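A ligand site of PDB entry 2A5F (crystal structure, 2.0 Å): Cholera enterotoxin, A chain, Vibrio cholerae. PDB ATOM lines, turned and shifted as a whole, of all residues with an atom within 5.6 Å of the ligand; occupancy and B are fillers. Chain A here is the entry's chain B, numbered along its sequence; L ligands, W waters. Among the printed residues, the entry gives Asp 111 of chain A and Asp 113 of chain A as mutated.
The backbone NH of Ser 11 lies within hydrogen-bond range of an oxygen (O5) of the ligand (3.2 Å). O6 of the ligand lies within hydrogen-bond range of OG of Ser 11, 2.6 Å away. The backbone NH (N) of Ala 9 is in hydrogen-bond range of an oxygen (O14) of the ligand (2.7 Å). N7 of the ligand is in hydrogen-bond range of O of Ala 9 (3.0 Å). An oxygen (O2) of the ligand is in salt-bridge range of the guanidinium group (NH1) of Arg 26 (2.7 Å). An oxygen (O8) of the ligand is in salt-bridge range of the guanidinium group of Arg 8. The backbone carbonyl oxygen (O) of Met 24 sits at hydrogen-bond distance from a nitrogen (N3) of the ligand. An oxygen (O13) of the ligand is in hydrogen-bond range of the side-chain carboxylate (OD1) of Asp 113 (3.1 Å). The side-chain carboxylate (OD2) of Asp 111 is in hydrogen-bond range of an oxygen (O13) of the ligand, at 3.4 Å.
NH1 of Arg 8 sits at hydrogen-bond distance from O of Ser 62. OD2 of Asp 10 lies within salt-bridge range of NH2 of Arg 8 (2.8 Å). The backbone carbonyl oxygen of Tyr 7 sits at hydrogen-bond distance from the backbone NH of Ser 64. OD2 of Asp 113 lies within hydrogen-bond range of N of Thr 63. OD1 of Asp 113 sits at hydrogen-bond distance from OG of Ser 62 (2.7 Å). The backbone carbonyl oxygen (O) of Val 114 sits at hydrogen-bond distance from the side-chain hydroxyl (OG1) of Thr 63, at 2.6 Å. NE of Arg 12 is in salt-bridge range of OD1 of Asp 10. NE2 of His 45 lies close to OG of Ser 62 (3.3 Å).
O of Tyr 7 touches O14 of the ligand (3.8 Å). CA of Asp 10 touches O5 of the ligand, 3.6 Å away. Arg 12 touches the ligand. Pro 25 touches the ligand. Val 54 touches the ligand. CB of Ser 62 touches O8 of the ligand (3.5 Å). Thr 63 touches the ligand. OG of Ser 64 touches C19 of the ligand, at 3.1 Å. Val 73 touches the ligand. Ile 77 touches the ligand. CD2 of Leu 78 touches O5 of the ligand, 3.6 Å away. Hydrophobic or aromatic side chains within 4 Å of the ligand: Ala 9, Val 54, Val 73, Ile 77 and Leu 78. Of the 26 residues printed, 18 come within 4 Å of the ligand.
Water W4 bridges O9 of the ligand (2.6 Å) and O of Ala 9 (2.9 Å). Water W6 lies within hydrogen-bond range of the side-chain carboxylate of Asp 111 and an oxygen (O12) of the ligand. Water W3 bridges the guanidinium group of Arg 26 and an oxygen (O4) of the ligand. Water W1 lies within hydrogen-bond range of OD1 of Asp 113 (2.7 Å), O13 of the ligand (3.4 Å) and NE2 of His 45 (3.4 Å).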
ATOM      1  N   TYR A   7      22.371   4.634 -13.536  1.00  0.00           N
ATOM      2  CA  TYR A   7      23.810   4.792 -13.487  1.00  0.00           C
ATOM      3  C   TYR A   7      24.172   6.251 -13.308  1.00  0.00           C
ATOM      4  O   TYR A   7      23.736   7.087 -14.070  1.00  0.00           O
ATOM      5  CB  TYR A   7      24.390   4.265 -14.804  1.00  0.00           C
ATOM      6  CG  TYR A   7      23.935   2.881 -15.102  1.00  0.00           C
ATOM      7  CD1 TYR A   7      22.720   2.663 -15.659  1.00  0.00           C
ATOM      8  CD2 TYR A   7      24.713   1.775 -14.732  1.00  0.00           C
ATOM      9  CE1 TYR A   7      22.261   1.394 -15.898  1.00  0.00           C
ATOM     10  CE2 TYR A   7      24.238   0.487 -14.933  1.00  0.00           C
ATOM     11  CZ  TYR A   7      23.019   0.296 -15.516  1.00  0.00           C
ATOM     12  OH  TYR A   7      22.528  -0.992 -15.788  1.00  0.00           O
ATOM     13  N   ARG A   8      24.978   6.553 -12.307  1.00  0.00           N
ATOM     14  CA  ARG A   8      25.416   7.918 -12.063  1.00  0.00           C
ATOM     15  C   ARG A   8      26.922   7.955 -12.044  1.00  0.00           C
ATOM     16  O   ARG A   8      27.563   7.242 -11.245  1.00  0.00           O
ATOM     17  CB  ARG A   8      24.873   8.460 -10.734  1.00  0.00           C
ATOM     18  CG  ARG A   8      25.500   9.766 -10.339  1.00  0.00           C
ATOM     19  CD  ARG A   8      24.898  10.427  -9.162  1.00  0.00           C
ATOM     20  NE  ARG A   8      25.729  11.566  -8.807  1.00  0.00           N
ATOM     21  CZ  ARG A   8      25.641  12.790  -9.329  1.00  0.00           C
ATOM     22  NH1 ARG A   8      24.677  13.101 -10.169  1.00  0.00           N
ATOM     23  NH2 ARG A   8      26.511  13.707  -8.979  1.00  0.00           N
ATOM     24  N   ALA A   9      27.485   8.774 -12.942  1.00  0.00           N
ATOM     25  CA  ALA A   9      28.900   9.119 -12.914  1.00  0.00           C
ATOM     26  C   ALA A   9      29.147  10.150 -11.840  1.00  0.00           C
ATOM     27  O   ALA A   9      28.456  11.156 -11.751  1.00  0.00           O
ATOM     28  CB  ALA A   9      29.352   9.666 -14.270  1.00  0.00           C
ATOM     29  N   ASP A  10      30.150   9.924 -11.027  1.00  0.00           N
ATOM     30  CA  ASP A  10      30.456  10.799  -9.898  1.00  0.00           C
ATOM     31  C   ASP A  10      31.938  10.641  -9.586  1.00  0.00           C
ATOM     32  O   ASP A  10      32.471   9.521  -9.630  1.00  0.00           O
ATOM     33  CB  ASP A  10      29.570  10.404  -8.684  1.00  0.00           C
ATOM     34  CG  ASP A  10      29.459  11.530  -7.611  1.00  0.00           C
ATOM     35  OD1 ASP A  10      30.470  11.833  -6.896  1.00  0.00           O
ATOM     36  OD2 ASP A  10      28.350  12.106  -7.526  1.00  0.00           O
ATOM     37  N   SER A  11      32.584  11.745  -9.254  1.00  0.00           N
ATOM     38  CA  SER A  11      34.024  11.744  -8.937  1.00  0.00           C
ATOM     39  C   SER A  11      34.319  11.354  -7.484  1.00  0.00           C
ATOM     40  O   SER A  11      35.453  11.006  -7.158  1.00  0.00           O
ATOM     41  CB  SER A  11      34.641  13.097  -9.234  1.00  0.00           C
ATOM     42  OG  SER A  11      34.264  14.099  -8.319  1.00  0.00           O
ATOM     43  N   ARG A  12      33.301  11.324  -6.626  1.00  0.00           N
ATOM     44  CA  ARG A  12      33.522  10.926  -5.234  1.00  0.00           C
ATOM     45  C   ARG A  12      33.620   9.400  -5.055  1.00  0.00           C
ATOM     46  O   ARG A  12      32.770   8.661  -5.538  1.00  0.00           O
ATOM     47  CB  ARG A  12      32.435  11.504  -4.318  1.00  0.00           C
ATOM     48  CG  ARG A  12      32.435  13.022  -4.308  1.00  0.00           C
ATOM     49  CD  ARG A  12      31.161  13.555  -3.660  1.00  0.00           C
ATOM     50  NE  ARG A  12      29.981  13.182  -4.415  1.00  0.00           N
ATOM     51  CZ  ARG A  12      28.743  13.256  -3.963  1.00  0.00           C
ATOM     52  NH1 ARG A  12      28.497  13.697  -2.735  1.00  0.00           N
ATOM     53  NH2 ARG A  12      27.751  12.902  -4.737  1.00  0.00           N
ATOM     54  N   GLU A  16      33.682   7.762   0.556  1.00  0.00           N
ATOM     55  CA  GLU A  16      33.111   9.071   0.814  1.00  0.00           C
ATOM     56  C   GLU A  16      31.599   9.029   0.653  1.00  0.00           C
ATOM     57  O   GLU A  16      30.868   9.636   1.427  1.00  0.00           O
ATOM     58  CB  GLU A  16      33.709  10.132  -0.087  1.00  0.00           C
ATOM     59  CG  GLU A  16      33.038  11.474   0.056  1.00  0.00           C
ATOM     60  CD  GLU A  16      33.682  12.550  -0.802  1.00  0.00           C
ATOM     61  OE1 GLU A  16      34.739  12.288  -1.404  1.00  0.00           O
ATOM     62  OE2 GLU A  16      33.148  13.685  -0.847  1.00  0.00           O
ATOM     63  N   MET A  24      23.737  12.509  -2.059  1.00  0.00           N
ATOM     64  CA  MET A  24      22.821  13.539  -1.548  1.00  0.00           C
ATOM     65  C   MET A  24      22.820  14.768  -2.455  1.00  0.00           C
ATOM     66  O   MET A  24      23.827  15.069  -3.097  1.00  0.00           O
ATOM     67  CB  MET A  24      23.196  13.918  -0.094  1.00  0.00           C
ATOM     68  CG  MET A  24      22.954  12.766   0.919  1.00  0.00           C
ATOM     69  SD  MET A  24      21.226  12.109   0.956  1.00  0.00           S
ATOM     70  CE  MET A  24      21.485  10.365   0.673  1.00  0.00           C
ATOM     71  N   PRO A  25      21.682  15.472  -2.511  1.00  0.00           N
ATOM     72  CA  PRO A  25      21.618  16.643  -3.355  1.00  0.00           C
ATOM     73  C   PRO A  25      22.481  17.758  -2.791  1.00  0.00           C
ATOM     74  O   PRO A  25      22.705  17.785  -1.574  1.00  0.00           O
ATOM     75  CB  PRO A  25      20.142  17.017  -3.349  1.00  0.00           C
ATOM     76  CG  PRO A  25      19.564  16.328  -2.166  1.00  0.00           C
ATOM     77  CD  PRO A  25      20.424  15.198  -1.811  1.00  0.00           C
ATOM     78  N   ARG A  26      22.935  18.655  -3.666  1.00  0.00           N
ATOM     79  CA  ARG A  26      23.702  19.836  -3.252  1.00  0.00           C
ATOM     80  C   ARG A  26      22.943  20.704  -2.273  1.00  0.00           C
ATOM     81  O   ARG A  26      23.511  21.252  -1.331  1.00  0.00           O
ATOM     82  CB  ARG A  26      24.012  20.703  -4.444  1.00  0.00           C
ATOM     83  CG  ARG A  26      24.902  20.062  -5.418  1.00  0.00           C
ATOM     84  CD  ARG A  26      25.377  21.122  -6.337  1.00  0.00           C
ATOM     85  NE  ARG A  26      26.413  20.627  -7.229  1.00  0.00           N
ATOM     86  CZ  ARG A  26      27.677  20.438  -6.890  1.00  0.00           C
ATOM     87  NH1 ARG A  26      28.546  20.033  -7.785  1.00  0.00           N
ATOM     88  NH2 ARG A  26      28.074  20.667  -5.642  1.00  0.00           N
ATOM     89  N   SER A  29      23.399  20.167   1.737  1.00  0.00           N
ATOM     90  CA  SER A  29      24.537  20.831   2.377  1.00  0.00           C
ATOM     91  C   SER A  29      24.279  22.305   2.536  1.00  0.00           C
ATOM     92  O   SER A  29      24.669  22.901   3.528  1.00  0.00           O
ATOM     93  CB  SER A  29      25.793  20.674   1.527  1.00  0.00           C
ATOM     94  OG  SER A  29      25.854  19.364   1.012  1.00  0.00           O
ATOM     95  N   HIS A  45      16.213  22.504 -11.902  1.00  0.00           N
ATOM     96  CA  HIS A  45      17.257  21.495 -11.894  1.00  0.00           C
ATOM     97  C   HIS A  45      17.764  21.235 -13.319  1.00  0.00           C
ATOM     98  O   HIS A  45      18.985  21.187 -13.554  1.00  0.00           O
ATOM     99  CB  HIS A  45      16.698  20.217 -11.252  1.00  0.00           C
ATOM    100  CG  HIS A  45      17.509  18.993 -11.539  1.00  0.00           C
ATOM    101  ND1 HIS A  45      18.732  18.757 -10.953  1.00  0.00           N
ATOM    102  CD2 HIS A  45      17.222  17.901 -12.278  1.00  0.00           C
ATOM    103  CE1 HIS A  45      19.181  17.585 -11.369  1.00  0.00           C
ATOM    104  NE2 HIS A  45      18.285  17.057 -12.183  1.00  0.00           N
ATOM    105  N   VAL A  54      25.031  23.917 -12.276  1.00  0.00           N
ATOM    106  CA  VAL A  54      24.173  23.308 -11.249  1.00  0.00           C
ATOM    107  C   VAL A  54      23.940  24.243 -10.043  1.00  0.00           C
ATOM    108  O   VAL A  54      24.889  24.803  -9.478  1.00  0.00           O
ATOM    109  CB  VAL A  54      24.721  21.954 -10.744  1.00  0.00           C
ATOM    110  CG1 VAL A  54      23.767  21.320  -9.700  1.00  0.00           C
ATOM    111  CG2 VAL A  54      24.945  20.996 -11.933  1.00  0.00           C
ATOM    112  N   VAL A  61      19.316  14.721  -7.536  1.00  0.00           N
ATOM    113  CA  VAL A  61      20.544  14.070  -7.989  1.00  0.00           C
ATOM    114  C   VAL A  61      20.318  13.355  -9.337  1.00  0.00           C
ATOM    115  O   VAL A  61      19.459  12.461  -9.470  1.00  0.00           O
ATOM    116  CB  VAL A  61      21.049  13.033  -6.936  1.00  0.00           C
ATOM    117  CG1 VAL A  61      22.261  12.277  -7.436  1.00  0.00           C
ATOM    118  CG2 VAL A  61      21.426  13.721  -5.645  1.00  0.00           C
ATOM    119  N   SER A  62      21.115  13.723 -10.341  1.00  0.00           N
ATOM    120  CA  SER A  62      20.951  13.193 -11.680  1.00  0.00           C
ATOM    121  C   SER A  62      21.544  11.774 -11.854  1.00  0.00           C
ATOM    122  O   SER A  62      22.555  11.453 -11.269  1.00  0.00           O
ATOM    123  CB  SER A  62      21.675  14.113 -12.675  1.00  0.00           C
ATOM    124  OG  SER A  62      21.084  15.368 -12.791  1.00  0.00           O
ATOM    125  N   THR A  63      20.873  10.956 -12.646  1.00  0.00           N
ATOM    126  CA  THR A  63      21.342   9.618 -13.038  1.00  0.00           C
ATOM    127  C   THR A  63      20.996   9.406 -14.526  1.00  0.00           C
ATOM    128  O   THR A  63      20.102  10.040 -15.093  1.00  0.00           O
ATOM    129  CB  THR A  63      20.662   8.440 -12.186  1.00  0.00           C
ATOM    130  OG1 THR A  63      19.354   8.154 -12.682  1.00  0.00           O
ATOM    131  CG2 THR A  63      20.570   8.737 -10.689  1.00  0.00           C
ATOM    132  N   SER A  64      21.697   8.448 -15.154  1.00  0.00           N
ATOM    133  CA  SER A  64      21.411   8.018 -16.506  1.00  0.00           C
ATOM    134  C   SER A  64      20.684   6.676 -16.541  1.00  0.00           C
ATOM    135  O   SER A  64      20.753   5.875 -15.617  1.00  0.00           O
ATOM    136  CB  SER A  64      22.719   7.869 -17.326  1.00  0.00           C
ATOM    137  OG  SER A  64      23.590   8.971 -17.098  1.00  0.00           O
ATOM    138  N   ALA A  70      25.960   7.024 -18.918  1.00  0.00           N
ATOM    139  CA  ALA A  70      26.696   7.498 -17.756  1.00  0.00           C
ATOM    140  C   ALA A  70      28.163   7.684 -18.048  1.00  0.00           C
ATOM    141  O   ALA A  70      28.795   8.593 -17.525  1.00  0.00           O
ATOM    142  CB  ALA A  70      26.509   6.626 -16.507  1.00  0.00           C
ATOM    143  N   VAL A  73      28.607  10.924 -20.096  1.00  0.00           N
ATOM    144  CA  VAL A  73      28.585  11.993 -19.103  1.00  0.00           C
ATOM    145  C   VAL A  73      29.892  12.105 -18.331  1.00  0.00           C
ATOM    146  O   VAL A  73      30.428  13.183 -18.185  1.00  0.00           O
ATOM    147  CB  VAL A  73      27.425  11.776 -18.081  1.00  0.00           C
ATOM    148  CG1 VAL A  73      27.537  12.736 -16.895  1.00  0.00           C
ATOM    149  CG2 VAL A  73      26.115  11.926 -18.771  1.00  0.00           C
ATOM    150  N   ILE A  77      31.599  15.678 -18.264  1.00  0.00           N
ATOM    151  CA  ILE A  77      31.570  16.436 -17.038  1.00  0.00           C
ATOM    152  C   ILE A  77      32.806  16.132 -16.220  1.00  0.00           C
ATOM    153  O   ILE A  77      33.413  17.043 -15.595  1.00  0.00           O
ATOM    154  CB  ILE A  77      30.247  16.090 -16.278  1.00  0.00           C
ATOM    155  CG1 ILE A  77      29.069  16.769 -16.965  1.00  0.00           C
ATOM    156  CG2 ILE A  77      30.324  16.488 -14.848  1.00  0.00           C
ATOM    157  N   LEU A  78      33.242  14.866 -16.216  1.00  0.00           N
ATOM    158  CA  LEU A  78      34.322  14.459 -15.332  1.00  0.00           C
ATOM    159  C   LEU A  78      35.638  14.239 -16.072  1.00  0.00           C
ATOM    160  O   LEU A  78      36.505  13.537 -15.597  1.00  0.00           O
ATOM    161  CB  LEU A  78      33.934  13.227 -14.502  1.00  0.00           C
ATOM    162  CG  LEU A  78      32.670  13.429 -13.654  1.00  0.00           C
ATOM    163  CD1 LEU A  78      32.156  12.154 -12.982  1.00  0.00           C
ATOM    164  CD2 LEU A  78      32.964  14.503 -12.625  1.00  0.00           C
ATOM    165  N   HIS A  81      39.079  14.387 -14.265  1.00  0.00           N
ATOM    166  CA  HIS A  81      39.392  13.407 -13.211  1.00  0.00           C
ATOM    167  C   HIS A  81      40.007  12.137 -13.797  1.00  0.00           C
ATOM    168  O   HIS A  81      39.357  11.419 -14.553  1.00  0.00           O
ATOM    169  CB  HIS A  81      38.115  13.029 -12.426  1.00  0.00           C
ATOM    170  CG  HIS A  81      37.502  14.172 -11.678  1.00  0.00           C
ATOM    171  ND1 HIS A  81      37.792  14.433 -10.353  1.00  0.00           N
ATOM    172  CD2 HIS A  81      36.663  15.161 -12.077  1.00  0.00           C
ATOM    173  CE1 HIS A  81      37.136  15.517  -9.969  1.00  0.00           C
ATOM    174  NE2 HIS A  81      36.452  15.984 -11.000  1.00  0.00           N
ATOM    175  N   ASP A 111      20.302  15.420 -22.193  1.00  0.00           N
ATOM    176  CA  ASP A 111      20.769  14.922 -20.901  1.00  0.00           C
ATOM    177  C   ASP A 111      20.185  13.544 -20.609  1.00  0.00           C
ATOM    178  O   ASP A 111      20.821  12.770 -19.920  1.00  0.00           O
ATOM    179  CB  ASP A 111      20.421  15.869 -19.752  1.00  0.00           C
ATOM    180  CG  ASP A 111      21.173  17.207 -19.809  1.00  0.00           C
ATOM    181  OD1 ASP A 111      22.303  17.239 -20.324  1.00  0.00           O
ATOM    182  OD2 ASP A 111      20.599  18.230 -19.294  1.00  0.00           O
ATOM    183  N   GLN A 112      18.994  13.235 -21.120  1.00  0.00           N
ATOM    184  CA  GLN A 112      18.250  11.984 -20.796  1.00  0.00           C
ATOM    185  C   GLN A 112      18.342  11.560 -19.305  1.00  0.00           C
ATOM    186  O   GLN A 112      18.762  10.453 -18.961  1.00  0.00           O
ATOM    187  CB  GLN A 112      18.629  10.847 -21.732  1.00  0.00           C
ATOM    188  CG  GLN A 112      18.545  11.275 -23.212  1.00  0.00           C
ATOM    189  CD  GLN A 112      17.691  10.346 -24.090  1.00  0.00           C
ATOM    190  OE1 GLN A 112      16.887  10.828 -24.925  1.00  0.00           O
ATOM    191  NE2 GLN A 112      17.868   9.037 -23.938  1.00  0.00           N
ATOM    192  N   ASP A 113      17.914  12.467 -18.425  1.00  0.00           N
ATOM    193  CA  ASP A 113      18.225  12.399 -17.011  1.00  0.00           C
ATOM    194  C   ASP A 113      17.043  11.699 -16.289  1.00  0.00           C
ATOM    195  O   ASP A 113      15.876  11.998 -16.552  1.00  0.00           O
ATOM    196  CB  ASP A 113      18.489  13.851 -16.559  1.00  0.00           C
ATOM    197  CG  ASP A 113      18.834  14.016 -15.088  1.00  0.00           C
ATOM    198  OD1 ASP A 113      19.251  15.152 -14.698  1.00  0.00           O
ATOM    199  OD2 ASP A 113      18.679  13.079 -14.284  1.00  0.00           O
ATOM    200  N   VAL A 114      17.349  10.724 -15.447  1.00  0.00           N
ATOM    201  CA  VAL A 114      16.395  10.294 -14.410  1.00  0.00           C
ATOM    202  C   VAL A 114      16.912  10.786 -13.061  1.00  0.00           C
ATOM    203  O   VAL A 114      18.003  10.407 -12.598  1.00  0.00           O
ATOM    204  CB  VAL A 114      16.173   8.773 -14.419  1.00  0.00           C
ATOM    205  CG1 VAL A 114      15.281   8.346 -13.272  1.00  0.00           C
ATOM    206  CG2 VAL A 114      15.552   8.329 -15.698  1.00  0.00           C
HETATM  207  P1  LIG L   1      26.661  17.410 -10.068  1.00  0.00           P
HETATM  208  O1  LIG L   1      25.681  16.683  -9.190  1.00  0.00           O
HETATM  209  O2  LIG L   1      26.891  18.767  -9.579  1.00  0.00           O
HETATM  210  O3  LIG L   1      28.032  16.522  -9.984  1.00  0.00           O
HETATM  211  C1  LIG L   1      29.299  17.043 -10.381  1.00  0.00           C
HETATM  212  C2  LIG L   1      30.294  16.733  -9.257  1.00  0.00           C
HETATM  213  O4  LIG L   1      30.062  17.542  -8.122  1.00  0.00           O
HETATM  214  C3  LIG L   1      30.250  15.288  -8.770  1.00  0.00           C
HETATM  215  O5  LIG L   1      30.902  14.399  -9.649  1.00  0.00           O
HETATM  216  C4  LIG L   1      30.882  15.434  -7.406  1.00  0.00           C
HETATM  217  O6  LIG L   1      32.316  15.531  -7.469  1.00  0.00           O
HETATM  218  C5  LIG L   1      30.306  16.760  -6.974  1.00  0.00           C
HETATM  219  N1  LIG L   1      29.028  16.642  -6.239  1.00  0.00           N
HETATM  220  C6  LIG L   1      27.763  16.344  -6.697  1.00  0.00           C
HETATM  221  N2  LIG L   1      26.925  16.380  -5.648  1.00  0.00           N
HETATM  222  C7  LIG L   1      27.650  16.690  -4.533  1.00  0.00           C
HETATM  223  C8  LIG L   1      27.304  16.845  -3.188  1.00  0.00           C
HETATM  224  N3  LIG L   1      26.031  16.736  -2.785  1.00  0.00           N
HETATM  225  N4  LIG L   1      28.311  17.178  -2.295  1.00  0.00           N
HETATM  226  C9  LIG L   1      29.634  17.339  -2.710  1.00  0.00           C
HETATM  227  N5  LIG L   1      29.964  17.170  -4.048  1.00  0.00           N
HETATM  228  C10 LIG L   1      28.970  16.866  -4.906  1.00  0.00           C
HETATM  229  O7  LIG L   1      26.360  17.383 -11.628  1.00  0.00           O
HETATM  230  P2  LIG L   1      25.964  16.043 -12.436  1.00  0.00           P
HETATM  231  O8  LIG L   1      24.864  15.326 -11.779  1.00  0.00           O
HETATM  232  O9  LIG L   1      27.275  15.469 -12.676  1.00  0.00           O
HETATM  233  O10 LIG L   1      25.155  16.596 -13.716  1.00  0.00           O
HETATM  234  C11 LIG L   1      25.697  17.514 -14.618  1.00  0.00           C
HETATM  235  C12 LIG L   1      24.911  17.381 -15.926  1.00  0.00           C
HETATM  236  O11 LIG L   1      24.913  16.047 -16.414  1.00  0.00           O
HETATM  237  C13 LIG L   1      23.435  17.771 -15.786  1.00  0.00           C
HETATM  238  O12 LIG L   1      23.086  18.382 -16.990  1.00  0.00           O
HETATM  239  C14 LIG L   1      22.644  16.478 -15.801  1.00  0.00           C
HETATM  240  O13 LIG L   1      21.422  16.590 -16.468  1.00  0.00           O
HETATM  241  C15 LIG L   1      23.567  15.567 -16.607  1.00  0.00           C
HETATM  242  N6  LIG L   1      23.470  14.166 -16.172  1.00  0.00           N
HETATM  243  C16 LIG L   1      24.396  13.677 -15.269  1.00  0.00           C
HETATM  244  C17 LIG L   1      24.363  12.332 -14.877  1.00  0.00           C
HETATM  245  C18 LIG L   1      25.435  11.723 -14.035  1.00  0.00           C
HETATM  246  O14 LIG L   1      25.655  10.383 -14.182  1.00  0.00           O
HETATM  247  N7  LIG L   1      26.153  12.396 -13.156  1.00  0.00           N
HETATM  248  C19 LIG L   1      23.386  11.520 -15.421  1.00  0.00           C
HETATM  249  C20 LIG L   1      22.475  12.024 -16.342  1.00  0.00           C
HETATM  250  C21 LIG L   1      22.521  13.349 -16.707  1.00  0.00           C
HETATM  251  O   HOH W   1      18.216  17.458 -15.602  1.00  0.00           O
HETATM  252  O   HOH W   2      34.493  17.924  -8.427  1.00  0.00           O
HETATM  253  O   HOH W   3      31.501  20.111  -6.765  1.00  0.00           O
HETATM  254  O   HOH W   4      29.231  13.995 -11.669  1.00  0.00           O
HETATM  255  O   HOH W   5      24.493  15.629  -6.783  1.00  0.00           O
HETATM  256  O   HOH W   6      20.771  20.419 -17.476  1.00  0.00           O
